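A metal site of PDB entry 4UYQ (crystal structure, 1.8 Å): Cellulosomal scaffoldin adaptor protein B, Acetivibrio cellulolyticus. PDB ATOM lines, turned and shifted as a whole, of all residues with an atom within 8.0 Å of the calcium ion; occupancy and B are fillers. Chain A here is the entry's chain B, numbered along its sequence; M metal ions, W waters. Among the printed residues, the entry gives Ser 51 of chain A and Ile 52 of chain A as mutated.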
ATOM      1  N   ILE A  21      -0.463 -11.791 -27.609  1.00  0.00           N
ATOM      2  CA  ILE A  21       0.078 -12.358 -26.387  1.00  0.00           C
ATOM      3  C   ILE A  21      -0.987 -12.733 -25.386  1.00  0.00           C
ATOM      4  O   ILE A  21      -1.052 -13.894 -24.863  1.00  0.00           O
ATOM      5  CB  ILE A  21       1.129 -11.402 -25.796  1.00  0.00           C
ATOM      6  CG1 ILE A  21       2.310 -11.183 -26.765  1.00  0.00           C
ATOM      7  CG2 ILE A  21       1.590 -11.853 -24.406  1.00  0.00           C
ATOM      8  CD1 ILE A  21       3.348 -10.194 -26.259  1.00  0.00           C
ATOM      9  N   MET A  38       7.663 -16.322 -30.483  1.00  0.00           N
ATOM     10  CA  MET A  38       7.862 -16.745 -29.078  1.00  0.00           C
ATOM     11  C   MET A  38       9.013 -16.012 -28.376  1.00  0.00           C
ATOM     12  O   MET A  38       8.934 -15.660 -27.211  1.00  0.00           O
ATOM     13  CB  MET A  38       8.151 -18.258 -29.018  1.00  0.00           C
ATOM     14  CG  MET A  38       7.631 -18.961 -27.795  1.00  0.00           C
ATOM     15  SD  MET A  38       5.816 -18.929 -27.588  1.00  0.00           S
ATOM     16  CE  MET A  38       5.218 -19.524 -29.149  1.00  0.00           C
ATOM     17  N   ALA A  41       7.823 -12.473 -27.805  1.00  0.00           N
ATOM     18  CA  ALA A  41       6.762 -12.392 -26.833  1.00  0.00           C
ATOM     19  C   ALA A  41       7.157 -12.334 -25.352  1.00  0.00           C
ATOM     20  O   ALA A  41       6.436 -11.740 -24.513  1.00  0.00           O
ATOM     21  CB  ALA A  41       5.778 -13.544 -27.068  1.00  0.00           C
ATOM     22  N   ASP A  42       8.283 -12.954 -25.014  1.00  0.00           N
ATOM     23  CA  ASP A  42       8.780 -12.973 -23.652  1.00  0.00           C
ATOM     24  C   ASP A  42       9.533 -11.697 -23.328  1.00  0.00           C
ATOM     25  O   ASP A  42      10.782 -11.634 -23.313  1.00  0.00           O
ATOM     26  CB  ASP A  42       9.640 -14.247 -23.400  1.00  0.00           C
ATOM     27  CG  ASP A  42      10.111 -14.342 -21.963  1.00  0.00           C
ATOM     28  OD1 ASP A  42       9.621 -13.548 -21.099  1.00  0.00           O
ATOM     29  OD2 ASP A  42      10.991 -15.194 -21.707  1.00  0.00           O
ATOM     30  N   VAL A  43       8.771 -10.631 -23.139  1.00  0.00           N
ATOM     31  CA  VAL A  43       9.343  -9.366 -22.903  1.00  0.00           C
ATOM     32  C   VAL A  43       9.723  -9.118 -21.434  1.00  0.00           C
ATOM     33  O   VAL A  43      10.504  -8.149 -21.230  1.00  0.00           O
ATOM     34  CB  VAL A  43       8.499  -8.239 -23.454  1.00  0.00           C
ATOM     35  CG1 VAL A  43       8.465  -8.383 -25.007  1.00  0.00           C
ATOM     36  CG2 VAL A  43       7.122  -8.270 -22.825  1.00  0.00           C
ATOM     37  N   ASP A  44       9.243  -9.916 -20.444  1.00  0.00           N
ATOM     38  CA  ASP A  44       9.703  -9.677 -19.069  1.00  0.00           C
ATOM     39  C   ASP A  44      10.992 -10.462 -18.811  1.00  0.00           C
ATOM     40  O   ASP A  44      11.732 -10.121 -17.904  1.00  0.00           O
ATOM     41  CB  ASP A  44       8.643  -9.906 -18.017  1.00  0.00           C
ATOM     42  CG  ASP A  44       8.397 -11.336 -17.735  1.00  0.00           C
ATOM     43  OD1 ASP A  44       8.813 -12.200 -18.585  1.00  0.00           O
ATOM     44  OD2 ASP A  44       7.788 -11.573 -16.642  1.00  0.00           O
ATOM     45  N   GLY A  45      11.269 -11.361 -19.748  1.00  0.00           N
ATOM     46  CA  GLY A  45      12.512 -12.059 -19.827  1.00  0.00           C
ATOM     47  C   GLY A  45      12.635 -13.161 -18.792  1.00  0.00           C
ATOM     48  O   GLY A  45      13.739 -13.608 -18.528  1.00  0.00           O
ATOM     49  N   ASN A  46      11.522 -13.622 -18.247  1.00  0.00           N
ATOM     50  CA  ASN A  46      11.528 -14.723 -17.266  1.00  0.00           C
ATOM     51  C   ASN A  46      11.392 -16.143 -17.829  1.00  0.00           C
ATOM     52  O   ASN A  46      11.307 -17.078 -17.086  1.00  0.00           O
ATOM     53  CB  ASN A  46      10.497 -14.444 -16.175  1.00  0.00           C
ATOM     54  CG  ASN A  46      10.959 -13.382 -15.202  1.00  0.00           C
ATOM     55  OD1 ASN A  46      12.089 -13.415 -14.729  1.00  0.00           O
ATOM     56  ND2 ASN A  46      10.109 -12.433 -14.894  1.00  0.00           N
ATOM     57  N   GLY A  47      11.408 -16.313 -19.152  1.00  0.00           N
ATOM     58  CA  GLY A  47      11.435 -17.651 -19.748  1.00  0.00           C
ATOM     59  C   GLY A  47      10.102 -18.277 -20.126  1.00  0.00           C
ATOM     60  O   GLY A  47      10.084 -19.384 -20.616  1.00  0.00           O
ATOM     61  N   SER A  48       8.980 -17.567 -19.961  1.00  0.00           N
ATOM     62  CA  SER A  48       7.658 -18.095 -20.358  1.00  0.00           C
ATOM     63  C   SER A  48       6.838 -16.909 -20.836  1.00  0.00           C
ATOM     64  O   SER A  48       7.282 -15.790 -20.667  1.00  0.00           O
ATOM     65  CB  SER A  48       6.920 -18.743 -19.159  1.00  0.00           C
ATOM     66  OG  SER A  48       6.989 -17.929 -17.996  1.00  0.00           O
ATOM     67  N   ILE A  49       5.668 -17.155 -21.396  1.00  0.00           N
ATOM     68  CA  ILE A  49       4.740 -16.105 -21.851  1.00  0.00           C
ATOM     69  C   ILE A  49       3.565 -16.048 -20.913  1.00  0.00           C
ATOM     70  O   ILE A  49       2.848 -17.057 -20.690  1.00  0.00           O
ATOM     71  CB  ILE A  49       4.353 -16.374 -23.308  1.00  0.00           C
ATOM     72  CG1 ILE A  49       5.649 -16.361 -24.120  1.00  0.00           C
ATOM     73  CG2 ILE A  49       3.411 -15.300 -23.867  1.00  0.00           C
ATOM     74  CD1 ILE A  49       5.461 -16.951 -25.464  1.00  0.00           C
ATOM     75  N   LYS A  50       3.373 -14.894 -20.294  1.00  0.00           N
ATOM     76  CA  LYS A  50       2.406 -14.798 -19.204  1.00  0.00           C
ATOM     77  C   LYS A  50       1.627 -13.515 -19.364  1.00  0.00           C
ATOM     78  O   LYS A  50       2.017 -12.690 -20.162  1.00  0.00           O
ATOM     79  CB  LYS A  50       3.171 -14.797 -17.874  1.00  0.00           C
ATOM     80  CG  LYS A  50       3.716 -16.195 -17.544  1.00  0.00           C
ATOM     81  CD  LYS A  50       4.487 -16.232 -16.266  1.00  0.00           C
ATOM     82  CE  LYS A  50       3.582 -16.117 -15.063  1.00  0.00           C
ATOM     83  NZ  LYS A  50       4.350 -16.273 -13.805  1.00  0.00           N
ATOM     84  N   SER A  51       0.612 -13.308 -18.522  1.00  0.00           N
ATOM     85  CA  SER A  51      -0.208 -12.159 -18.682  1.00  0.00           C
ATOM     86  C   SER A  51       0.554 -10.831 -18.680  1.00  0.00           C
ATOM     87  O   SER A  51       0.178  -9.882 -19.385  1.00  0.00           O
ATOM     88  CB  SER A  51      -1.217 -12.066 -17.515  1.00  0.00           C
ATOM     89  OG  SER A  51      -2.272 -12.970 -17.775  1.00  0.00           O
ATOM     90  N   ILE A  52       1.535 -10.733 -17.761  1.00  0.00           N
ATOM     91  CA  ILE A  52       2.383  -9.523 -17.696  1.00  0.00           C
ATOM     92  C   ILE A  52       3.063  -9.129 -19.036  1.00  0.00           C
ATOM     93  O   ILE A  52       3.256  -7.917 -19.300  1.00  0.00           O
ATOM     94  CB  ILE A  52       3.359  -9.632 -16.526  1.00  0.00           C
ATOM     95  CG1 ILE A  52       4.046  -8.291 -16.209  1.00  0.00           C
ATOM     96  CG2 ILE A  52       4.380 -10.757 -16.776  1.00  0.00           C
ATOM     97  CD1 ILE A  52       3.060  -7.243 -15.796  1.00  0.00           C
ATOM     98  N   ASP A  53       3.411 -10.114 -19.849  1.00  0.00           N
ATOM     99  CA  ASP A  53       4.009  -9.843 -21.186  1.00  0.00           C
ATOM    100  C   ASP A  53       3.102  -8.922 -22.053  1.00  0.00           C
ATOM    101  O   ASP A  53       3.550  -7.933 -22.685  1.00  0.00           O
ATOM    102  CB  ASP A  53       4.399 -11.143 -21.842  1.00  0.00           C
ATOM    103  CG  ASP A  53       5.552 -11.842 -21.072  1.00  0.00           C
ATOM    104  OD1 ASP A  53       6.647 -11.250 -20.923  1.00  0.00           O
ATOM    105  OD2 ASP A  53       5.343 -12.916 -20.514  1.00  0.00           O
ATOM    106  N   ALA A  54       1.815  -9.258 -22.041  1.00  0.00           N
ATOM    107  CA  ALA A  54       0.811  -8.483 -22.784  1.00  0.00           C
ATOM    108  C   ALA A  54       0.668  -7.070 -22.189  1.00  0.00           C
ATOM    109  O   ALA A  54       0.607  -6.102 -22.959  1.00  0.00           O
ATOM    110  CB  ALA A  54      -0.551  -9.221 -22.804  1.00  0.00           C
ATOM    111  N   LEU A  56       3.044  -5.367 -20.621  1.00  0.00           N
ATOM    112  CA  LEU A  56       4.263  -4.673 -20.975  1.00  0.00           C
ATOM    113  C   LEU A  56       4.270  -4.217 -22.415  1.00  0.00           C
ATOM    114  O   LEU A  56       4.650  -3.042 -22.662  1.00  0.00           O
ATOM    115  CB  LEU A  56       5.528  -5.524 -20.709  1.00  0.00           C
ATOM    116  CG  LEU A  56       5.862  -5.707 -19.212  1.00  0.00           C
ATOM    117  CD1 LEU A  56       6.846  -6.860 -19.032  1.00  0.00           C
ATOM    118  CD2 LEU A  56       6.407  -4.429 -18.606  1.00  0.00           C
ATOM    119  N   VAL A  70      13.353  -7.550 -20.515  1.00  0.00           N
ATOM    120  CA  VAL A  70      14.276  -8.531 -21.078  1.00  0.00           C
ATOM    121  C   VAL A  70      15.542  -7.841 -21.639  1.00  0.00           C
ATOM    122  O   VAL A  70      16.622  -8.472 -21.865  1.00  0.00           O
ATOM    123  CB  VAL A  70      13.600  -9.369 -22.180  1.00  0.00           C
ATOM    124  CG1 VAL A  70      13.241  -8.534 -23.407  1.00  0.00           C
ATOM    125  CG2 VAL A  70      14.482 -10.524 -22.684  1.00  0.00           C
HETATM  126 CA    CA M   1       7.559 -13.564 -20.025  1.00  0.00          CA
HETATM  127  O   HOH W   1       7.780 -15.247 -17.936  1.00  0.00           O
HETATM  128  O   HOH W   2       6.183 -13.613 -17.801  1.00  0.00           O
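The backbone NH (N) of Lys 50 sits close to the side-chain carboxylate (OD2) of Asp 53, 2.8 Å away. The side-chain carboxylate of Asp 42 lies close to the backbone NH of Asn 46, at 3.4 Å. The side-chain carboxylate (OD1) of Asp 42 lies close to the backbone NH (N) of Gly 45, at 3.1 Å. The side-chain carboxylate (OD2) of Asp 42 is in hydrogen-bond range of the backbone NH (N) of Gly 47 (2.8 Å). ND2 of Asn 46 is in hydrogen-bond range of OD2 of Asp 44 (3.0 Å). The backbone NH (N) of Val 43 lies close to the side-chain carboxylate (OD1) of Asp 53.
Of the 18 residues printed, 4 come within 4 Å of the calcium ion. The nearest printed residue that does not touch the calcium ion is Ile 49 (4.2 Å).
The calcium ion is bound by OD1 of Asp 42, O of Ser 48, OD1 of Asp 44, OD2 of Asp 53, water W2, OD1 of Asp 53 and water W1. The calcium ion has seven donor atoms within binding distance.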
